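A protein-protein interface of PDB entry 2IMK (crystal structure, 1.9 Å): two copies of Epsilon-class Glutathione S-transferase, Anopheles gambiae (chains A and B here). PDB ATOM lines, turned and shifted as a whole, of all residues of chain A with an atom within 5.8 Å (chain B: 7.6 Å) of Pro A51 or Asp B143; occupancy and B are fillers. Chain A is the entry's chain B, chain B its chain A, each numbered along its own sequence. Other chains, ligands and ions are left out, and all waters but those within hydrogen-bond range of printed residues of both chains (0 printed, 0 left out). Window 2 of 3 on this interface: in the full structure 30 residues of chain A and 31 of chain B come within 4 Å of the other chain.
Among the printed residues, pairs that only touch across the chains: Pro A51 with Asp B143 (3.7 Å), Gln A52 with Leu B140 (3.7 Å) and His A53 with Leu B140 (3.8 Å).
Hydrophobic or aromatic side chains of chain A that line the printed part of chain B: Pro A51 and His A53.
Among the printed residues, 5 pairs touch across the chains.
Among the printed residues, no Asp or Glu carboxylate lies within 4 Å of a Lys or Arg side-chain nitrogen of the other chain.
Pro A51 touches just one residue of chain B: Asp B143 (3.7 Å).
Of chain A, only Pro A51 (3.7 Å) comes within 4 Å of Asp B143.
Of the printed residues of chain B, Gln A52 touches Leu B140 (3.7 Å) and Thr B144 (2.9 Å).
Of the printed residues of chain A, Thr B144 touches Gln A52 (2.9 Å).
Printed residues of chain A within 4 Å of Lys B136: His A53.
Of the printed residues of chain B, His A53 touches Lys B136 and Leu B140.
Thr A66 touches none of the printed residues of chain B.
Lys A48 touches none of the printed residues of chain B.
The nearest printed residue of chain B that does not touch Gln A52 is Asp B143 (5.6 Å).
NZ of Lys B136 lies within salt-bridge range of OE1 of Glu B139.
The backbone carbonyl oxygen of Leu B140 lies within hydrogen-bond range of the side-chain hydroxyl of Thr B144 (2.7 Å).
ND2 of Asn A50 lies close to N of Gln A52 (3.3 Å).
No position is printed for both chains.
Of the 5 pairs that touch across the chains among the printed residues, none has its exchanged pair printed and touching as well.
The side-chain amino group (NZ) of Lys B136 sits at hydrogen-bond distance from a ring nitrogen (NE2) of His A53 (3.5 Å).
OG1 of Thr B144 lies within hydrogen-bond range of OE1 of Gln A52 (2.9 Å).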
ATOM      1  N   PHE A  46     -11.792  -9.363   9.635  1.00  0.00           N
ATOM      2  CA  PHE A  46     -12.573  -8.756   8.576  1.00  0.00           C
ATOM      3  C   PHE A  46     -12.654  -9.580   7.272  1.00  0.00           C
ATOM      4  O   PHE A  46     -13.709  -9.622   6.644  1.00  0.00           O
ATOM      5  CB  PHE A  46     -12.151  -7.304   8.302  1.00  0.00           C
ATOM      6  CG  PHE A  46     -13.142  -6.568   7.416  1.00  0.00           C
ATOM      7  CD1 PHE A  46     -14.393  -6.182   7.915  1.00  0.00           C
ATOM      8  CD2 PHE A  46     -12.872  -6.367   6.067  1.00  0.00           C
ATOM      9  CE1 PHE A  46     -15.358  -5.578   7.100  1.00  0.00           C
ATOM     10  CE2 PHE A  46     -13.803  -5.746   5.263  1.00  0.00           C
ATOM     11  CZ  PHE A  46     -15.051  -5.349   5.788  1.00  0.00           C
ATOM     12  N   VAL A  47     -11.559 -10.237   6.879  1.00  0.00           N
ATOM     13  CA  VAL A  47     -11.549 -11.105   5.685  1.00  0.00           C
ATOM     14  C   VAL A  47     -12.513 -12.303   5.738  1.00  0.00           C
ATOM     15  O   VAL A  47     -13.000 -12.748   4.689  1.00  0.00           O
ATOM     16  CB  VAL A  47     -10.120 -11.569   5.307  1.00  0.00           C
ATOM     17  CG1 VAL A  47     -10.165 -12.594   4.178  1.00  0.00           C
ATOM     18  CG2 VAL A  47      -9.305 -10.394   4.923  1.00  0.00           C
ATOM     19  N   LYS A  48     -12.766 -12.826   6.946  1.00  0.00           N
ATOM     20  CA  LYS A  48     -13.767 -13.877   7.172  1.00  0.00           C
ATOM     21  C   LYS A  48     -15.196 -13.374   6.986  1.00  0.00           C
ATOM     22  O   LYS A  48     -16.053 -14.124   6.568  1.00  0.00           O
ATOM     23  CB  LYS A  48     -13.667 -14.477   8.589  1.00  0.00           C
ATOM     24  CG  LYS A  48     -12.263 -14.879   9.059  1.00  0.00           C
ATOM     25  CD  LYS A  48     -12.300 -15.123  10.582  1.00  0.00           C
ATOM     26  CE  LYS A  48     -10.970 -15.711  11.135  1.00  0.00           C
ATOM     27  NZ  LYS A  48     -11.065 -17.205  11.259  1.00  0.00           N
ATOM     28  N   LEU A  49     -15.451 -12.111   7.320  1.00  0.00           N
ATOM     29  CA  LEU A  49     -16.749 -11.439   7.056  1.00  0.00           C
ATOM     30  C   LEU A  49     -16.935 -11.218   5.561  1.00  0.00           C
ATOM     31  O   LEU A  49     -17.992 -11.481   4.995  1.00  0.00           O
ATOM     32  CB  LEU A  49     -16.776 -10.088   7.796  1.00  0.00           C
ATOM     33  CG  LEU A  49     -17.591  -9.931   9.072  1.00  0.00           C
ATOM     34  CD1 LEU A  49     -17.488 -11.136   9.976  1.00  0.00           C
ATOM     35  CD2 LEU A  49     -17.278  -8.640   9.756  1.00  0.00           C
ATOM     36  N   ASN A  50     -15.884 -10.738   4.907  1.00  0.00           N
ATOM     37  CA  ASN A  50     -15.952 -10.389   3.495  1.00  0.00           C
ATOM     38  C   ASN A  50     -14.667 -10.807   2.751  1.00  0.00           C
ATOM     39  O   ASN A  50     -13.648 -10.137   2.873  1.00  0.00           O
ATOM     40  CB  ASN A  50     -16.207  -8.878   3.403  1.00  0.00           C
ATOM     41  CG  ASN A  50     -16.514  -8.393   2.006  1.00  0.00           C
ATOM     42  OD1 ASN A  50     -16.544  -7.147   1.773  1.00  0.00           O
ATOM     43  ND2 ASN A  50     -16.795  -9.332   1.065  1.00  0.00           N
ATOM     44  N   PRO A  51     -14.713 -11.923   1.991  1.00  0.00           N
ATOM     45  CA  PRO A  51     -13.570 -12.331   1.135  1.00  0.00           C
ATOM     46  C   PRO A  51     -13.161 -11.324   0.030  1.00  0.00           C
ATOM     47  O   PRO A  51     -12.052 -11.424  -0.489  1.00  0.00           O
ATOM     48  CB  PRO A  51     -14.063 -13.625   0.467  1.00  0.00           C
ATOM     49  CG  PRO A  51     -15.622 -13.491   0.496  1.00  0.00           C
ATOM     50  CD  PRO A  51     -15.833 -12.880   1.888  1.00  0.00           C
ATOM     51  N   GLN A  52     -14.049 -10.410  -0.353  1.00  0.00           N
ATOM     52  CA  GLN A  52     -13.693  -9.359  -1.287  1.00  0.00           C
ATOM     53  C   GLN A  52     -13.060  -8.220  -0.528  1.00  0.00           C
ATOM     54  O   GLN A  52     -12.627  -7.209  -1.126  1.00  0.00           O
ATOM     55  CB  GLN A  52     -14.914  -8.910  -2.107  1.00  0.00           C
ATOM     56  CG  GLN A  52     -15.398  -9.991  -3.151  1.00  0.00           C
ATOM     57  CD  GLN A  52     -16.809  -9.788  -3.694  1.00  0.00           C
ATOM     58  OE1 GLN A  52     -17.403 -10.718  -4.320  1.00  0.00           O
ATOM     59  NE2 GLN A  52     -17.375  -8.603  -3.468  1.00  0.00           N
ATOM     60  N   HIS A  53     -13.009  -8.361   0.807  1.00  0.00           N
ATOM     61  CA  HIS A  53     -12.392  -7.340   1.662  1.00  0.00           C
ATOM     62  C   HIS A  53     -12.758  -5.844   1.322  1.00  0.00           C
ATOM     63  O   HIS A  53     -11.918  -4.954   1.342  1.00  0.00           O
ATOM     64  CB  HIS A  53     -10.854  -7.614   1.832  1.00  0.00           C
ATOM     65  CG  HIS A  53     -10.103  -7.800   0.539  1.00  0.00           C
ATOM     66  ND1 HIS A  53      -9.575  -6.740  -0.176  1.00  0.00           N
ATOM     67  CD2 HIS A  53      -9.787  -8.923  -0.163  1.00  0.00           C
ATOM     68  CE1 HIS A  53      -8.996  -7.203  -1.273  1.00  0.00           C
ATOM     69  NE2 HIS A  53      -9.129  -8.521  -1.300  1.00  0.00           N
ATOM     70  N   THR A  66     -22.905  -8.262   2.575  1.00  0.00           N
ATOM     71  CA  THR A  66     -21.833  -7.461   1.912  1.00  0.00           C
ATOM     72  C   THR A  66     -22.419  -6.613   0.776  1.00  0.00           C
ATOM     73  O   THR A  66     -23.475  -6.949   0.244  1.00  0.00           O
ATOM     74  CB  THR A  66     -20.676  -8.338   1.342  1.00  0.00           C
ATOM     75  OG1 THR A  66     -21.159  -9.126   0.221  1.00  0.00           O
ATOM     76  CG2 THR A  66     -20.179  -9.297   2.463  1.00  0.00           C
ATOM     77  N   LYS B 136      -6.521  -8.877 -10.588  1.00  0.00           N
ATOM     78  CA  LYS B 136      -7.127  -8.708  -9.285  1.00  0.00           C
ATOM     79  C   LYS B 136      -8.655  -9.072  -9.256  1.00  0.00           C
ATOM     80  O   LYS B 136      -9.136  -9.687  -8.297  1.00  0.00           O
ATOM     81  CB  LYS B 136      -6.772  -7.318  -8.716  1.00  0.00           C
ATOM     82  CG  LYS B 136      -7.278  -7.146  -7.291  1.00  0.00           C
ATOM     83  CD  LYS B 136      -6.245  -7.496  -6.164  1.00  0.00           C
ATOM     84  CE  LYS B 136      -6.901  -7.510  -4.761  1.00  0.00           C
ATOM     85  NZ  LYS B 136      -7.719  -8.777  -4.457  1.00  0.00           N
ATOM     86  N   SER B 137      -9.369  -8.790 -10.330  1.00  0.00           N
ATOM     87  CA  SER B 137     -10.776  -9.150 -10.412  1.00  0.00           C
ATOM     88  C   SER B 137     -10.872 -10.702 -10.372  1.00  0.00           C
ATOM     89  O   SER B 137     -11.775 -11.227  -9.743  1.00  0.00           O
ATOM     90  CB  SER B 137     -11.424  -8.603 -11.687  1.00  0.00           C
ATOM     91  OG  SER B 137     -11.168  -9.420 -12.861  1.00  0.00           O
ATOM     92  N   TYR B 138      -9.933 -11.405 -11.040  1.00  0.00           N
ATOM     93  CA  TYR B 138      -9.960 -12.890 -11.053  1.00  0.00           C
ATOM     94  C   TYR B 138      -9.786 -13.441  -9.651  1.00  0.00           C
ATOM     95  O   TYR B 138     -10.399 -14.432  -9.268  1.00  0.00           O
ATOM     96  CB  TYR B 138      -8.864 -13.488 -11.968  1.00  0.00           C
ATOM     97  CG  TYR B 138      -8.956 -13.154 -13.452  1.00  0.00           C
ATOM     98  CD1 TYR B 138     -10.190 -12.847 -14.062  1.00  0.00           C
ATOM     99  CD2 TYR B 138      -7.800 -13.198 -14.258  1.00  0.00           C
ATOM    100  CE1 TYR B 138     -10.252 -12.635 -15.456  1.00  0.00           C
ATOM    101  CE2 TYR B 138      -7.841 -12.950 -15.640  1.00  0.00           C
ATOM    102  CZ  TYR B 138      -9.069 -12.650 -16.225  1.00  0.00           C
ATOM    103  OH  TYR B 138      -9.110 -12.426 -17.570  1.00  0.00           O
ATOM    104  N   GLU B 139      -8.914 -12.807  -8.884  1.00  0.00           N
ATOM    105  CA  GLU B 139      -8.569 -13.281  -7.564  1.00  0.00           C
ATOM    106  C   GLU B 139      -9.740 -13.092  -6.610  1.00  0.00           C
ATOM    107  O   GLU B 139     -10.041 -13.983  -5.808  1.00  0.00           O
ATOM    108  CB  GLU B 139      -7.313 -12.576  -7.077  1.00  0.00           C
ATOM    109  CG  GLU B 139      -6.918 -12.864  -5.566  1.00  0.00           C
ATOM    110  CD  GLU B 139      -5.683 -12.092  -5.121  1.00  0.00           C
ATOM    111  OE1 GLU B 139      -5.624 -11.655  -3.944  1.00  0.00           O
ATOM    112  OE2 GLU B 139      -4.764 -11.876  -5.956  1.00  0.00           O
ATOM    113  N   LEU B 140     -10.410 -11.968  -6.745  1.00  0.00           N
ATOM    114  CA  LEU B 140     -11.652 -11.699  -5.998  1.00  0.00           C
ATOM    115  C   LEU B 140     -12.775 -12.681  -6.362  1.00  0.00           C
ATOM    116  O   LEU B 140     -13.518 -13.170  -5.487  1.00  0.00           O
ATOM    117  CB  LEU B 140     -12.103 -10.221  -6.179  1.00  0.00           C
ATOM    118  CG  LEU B 140     -11.206  -9.041  -5.718  1.00  0.00           C
ATOM    119  CD1 LEU B 140     -11.629  -7.765  -6.437  1.00  0.00           C
ATOM    120  CD2 LEU B 140     -11.456  -8.810  -4.273  1.00  0.00           C
ATOM    121  N   LEU B 141     -12.946 -12.944  -7.639  1.00  0.00           N
ATOM    122  CA  LEU B 141     -13.944 -13.923  -8.021  1.00  0.00           C
ATOM    123  C   LEU B 141     -13.628 -15.337  -7.445  1.00  0.00           C
ATOM    124  O   LEU B 141     -14.506 -15.992  -6.880  1.00  0.00           O
ATOM    125  CB  LEU B 141     -14.093 -14.009  -9.531  1.00  0.00           C
ATOM    126  CG  LEU B 141     -14.971 -15.169  -9.953  1.00  0.00           C
ATOM    127  CD1 LEU B 141     -16.473 -14.983  -9.507  1.00  0.00           C
ATOM    128  CD2 LEU B 141     -14.929 -15.252 -11.451  1.00  0.00           C
ATOM    129  N   GLU B 142     -12.399 -15.795  -7.645  1.00  0.00           N
ATOM    130  CA  GLU B 142     -11.914 -17.064  -7.079  1.00  0.00           C
ATOM    131  C   GLU B 142     -12.196 -17.161  -5.531  1.00  0.00           C
ATOM    132  O   GLU B 142     -12.728 -18.178  -5.084  1.00  0.00           O
ATOM    133  CB  GLU B 142     -10.404 -17.273  -7.473  1.00  0.00           C
ATOM    134  CG  GLU B 142      -9.733 -18.480  -6.759  1.00  0.00           C
ATOM    135  CD  GLU B 142      -9.995 -19.706  -7.499  1.00  0.00           C
ATOM    136  OE1 GLU B 142     -10.430 -19.565  -8.658  1.00  0.00           O
ATOM    137  OE2 GLU B 142      -9.765 -20.821  -6.980  1.00  0.00           O
ATOM    138  N   ASP B 143     -11.927 -16.093  -4.742  1.00  0.00           N
ATOM    139  CA  ASP B 143     -12.183 -16.069  -3.273  1.00  0.00           C
ATOM    140  C   ASP B 143     -13.691 -16.059  -2.921  1.00  0.00           C
ATOM    141  O   ASP B 143     -14.140 -16.480  -1.831  1.00  0.00           O
ATOM    142  CB  ASP B 143     -11.490 -14.830  -2.628  1.00  0.00           C
ATOM    143  CG  ASP B 143      -9.920 -14.951  -2.598  1.00  0.00           C
ATOM    144  OD1 ASP B 143      -9.242 -13.960  -2.146  1.00  0.00           O
ATOM    145  OD2 ASP B 143      -9.334 -16.003  -3.068  1.00  0.00           O
ATOM    146  N   THR B 144     -14.496 -15.540  -3.847  1.00  0.00           N
ATOM    147  CA  THR B 144     -15.951 -15.518  -3.705  1.00  0.00           C
ATOM    148  C   THR B 144     -16.587 -16.895  -3.906  1.00  0.00           C
ATOM    149  O   THR B 144     -17.565 -17.235  -3.234  1.00  0.00           O
ATOM    150  CB  THR B 144     -16.512 -14.477  -4.677  1.00  0.00           C
ATOM    151  OG1 THR B 144     -15.931 -13.190  -4.333  1.00  0.00           O
ATOM    152  CG2 THR B 144     -18.040 -14.425  -4.629  1.00  0.00           C
ATOM    153  N   LEU B 145     -16.006 -17.722  -4.773  1.00  0.00           N
ATOM    154  CA  LEU B 145     -16.558 -19.053  -5.096  1.00  0.00           C
ATOM    155  C   LEU B 145     -16.301 -20.131  -4.023  1.00  0.00           C
ATOM    156  O   LEU B 145     -15.742 -21.206  -4.331  1.00  0.00           O
ATOM    157  CB  LEU B 145     -15.958 -19.519  -6.415  1.00  0.00           C
ATOM    158  CG  LEU B 145     -16.644 -19.069  -7.670  1.00  0.00           C
ATOM    159  CD1 LEU B 145     -15.695 -19.281  -8.923  1.00  0.00           C
ATOM    160  CD2 LEU B 145     -18.002 -19.751  -7.866  1.00  0.00           C
ATOM    161  N   VAL B 146     -16.713 -19.848  -2.787  1.00  0.00           N
ATOM    162  CA  VAL B 146     -16.737 -20.849  -1.666  1.00  0.00           C
ATOM    163  C   VAL B 146     -17.724 -22.019  -1.939  1.00  0.00           C
ATOM    164  O   VAL B 146     -17.414 -23.208  -1.698  1.00  0.00           O
ATOM    165  CB  VAL B 146     -16.954 -20.143  -0.276  1.00  0.00           C
ATOM    166  CG1 VAL B 146     -15.908 -19.088  -0.117  1.00  0.00           C
ATOM    167  CG2 VAL B 146     -18.330 -19.491  -0.120  1.00  0.00           C
ATOM    168  N   ASP B 147     -18.892 -21.673  -2.504  1.00  0.00           N
ATOM    169  CA  ASP B 147     -19.837 -22.604  -2.995  1.00  0.00           C
ATOM    170  C   ASP B 147     -19.660 -22.943  -4.503  1.00  0.00           C
ATOM    171  O   ASP B 147     -18.836 -22.332  -5.193  1.00  0.00           O
ATOM    172  CB  ASP B 147     -21.185 -21.965  -2.751  1.00  0.00           C
ATOM    173  CG  ASP B 147     -21.625 -22.119  -1.328  1.00  0.00           C
ATOM    174  OD1 ASP B 147     -22.036 -23.257  -1.021  1.00  0.00           O
ATOM    175  OD2 ASP B 147     -21.559 -21.149  -0.514  1.00  0.00           O
ATOM    176  N   LYS B 179      -3.676 -21.226 -10.719  1.00  0.00           N
ATOM    177  CA  LYS B 179      -3.912 -20.221  -9.661  1.00  0.00           C
ATOM    178  C   LYS B 179      -5.399 -19.949  -9.438  1.00  0.00           C
ATOM    179  O   LYS B 179      -5.821 -19.367  -8.441  1.00  0.00           O
ATOM    180  CB  LYS B 179      -3.203 -18.921 -10.013  1.00  0.00           C
ATOM    181  CG  LYS B 179      -1.663 -19.058 -10.004  1.00  0.00           C
ATOM    182  CD  LYS B 179      -0.997 -17.728  -9.629  1.00  0.00           C
ATOM    183  CE  LYS B 179       0.447 -17.643 -10.203  1.00  0.00           C
ATOM    184  NZ  LYS B 179       1.169 -16.347  -9.794  1.00  0.00           N
ATOM    185  N   HIS B 180      -6.213 -20.388 -10.360  1.00  0.00           N
ATOM    186  CA  HIS B 180      -7.661 -20.162 -10.212  1.00  0.00           C
ATOM    187  C   HIS B 180      -8.456 -21.498 -10.377  1.00  0.00           C
ATOM    188  O   HIS B 180      -9.277 -21.592 -11.273  1.00  0.00           O
ATOM    189  CB  HIS B 180      -8.157 -19.020 -11.172  1.00  0.00           C
ATOM    190  CG  HIS B 180      -7.371 -17.728 -11.054  1.00  0.00           C
ATOM    191  ND1 HIS B 180      -6.217 -17.491 -11.769  1.00  0.00           N
ATOM    192  CD2 HIS B 180      -7.524 -16.662 -10.232  1.00  0.00           C
ATOM    193  CE1 HIS B 180      -5.742 -16.294 -11.470  1.00  0.00           C
ATOM    194  NE2 HIS B 180      -6.489 -15.789 -10.506  1.00  0.00           N
ATOM    195  N   ARG B 182     -10.921 -22.826  -8.660  1.00  0.00           N
ATOM    196  CA  ARG B 182     -12.352 -22.691  -8.400  1.00  0.00           C
ATOM    197  C   ARG B 182     -13.115 -22.086  -9.581  1.00  0.00           C
ATOM    198  O   ARG B 182     -14.179 -22.569  -9.937  1.00  0.00           O
ATOM    199  CB  ARG B 182     -12.663 -21.853  -7.136  1.00  0.00           C
ATOM    200  CG  ARG B 182     -12.167 -22.439  -5.776  1.00  0.00           C
ATOM    201  CD  ARG B 182     -12.546 -21.452  -4.661  1.00  0.00           C
ATOM    202  NE  ARG B 182     -12.231 -21.905  -3.317  1.00  0.00           N
ATOM    203  CZ  ARG B 182     -12.226 -21.102  -2.254  1.00  0.00           C
ATOM    204  NH1 ARG B 182     -12.513 -19.801  -2.388  1.00  0.00           N
ATOM    205  NH2 ARG B 182     -11.901 -21.602  -1.061  1.00  0.00           N
ATOM    206  N   ILE B 183     -12.586 -21.021 -10.168  1.00  0.00           N
ATOM    207  CA  ILE B 183     -13.152 -20.462 -11.411  1.00  0.00           C
ATOM    208  C   ILE B 183     -13.175 -21.554 -12.479  1.00  0.00           C
ATOM    209  O   ILE B 183     -14.169 -21.731 -13.150  1.00  0.00           O
ATOM    210  CB  ILE B 183     -12.328 -19.236 -11.923  1.00  0.00           C
ATOM    211  CG1 ILE B 183     -12.477 -18.077 -10.937  1.00  0.00           C
ATOM    212  CG2 ILE B 183     -12.776 -18.800 -13.353  1.00  0.00           C
ATOM    213  CD1 ILE B 183     -11.487 -16.916 -11.275  1.00  0.00           C
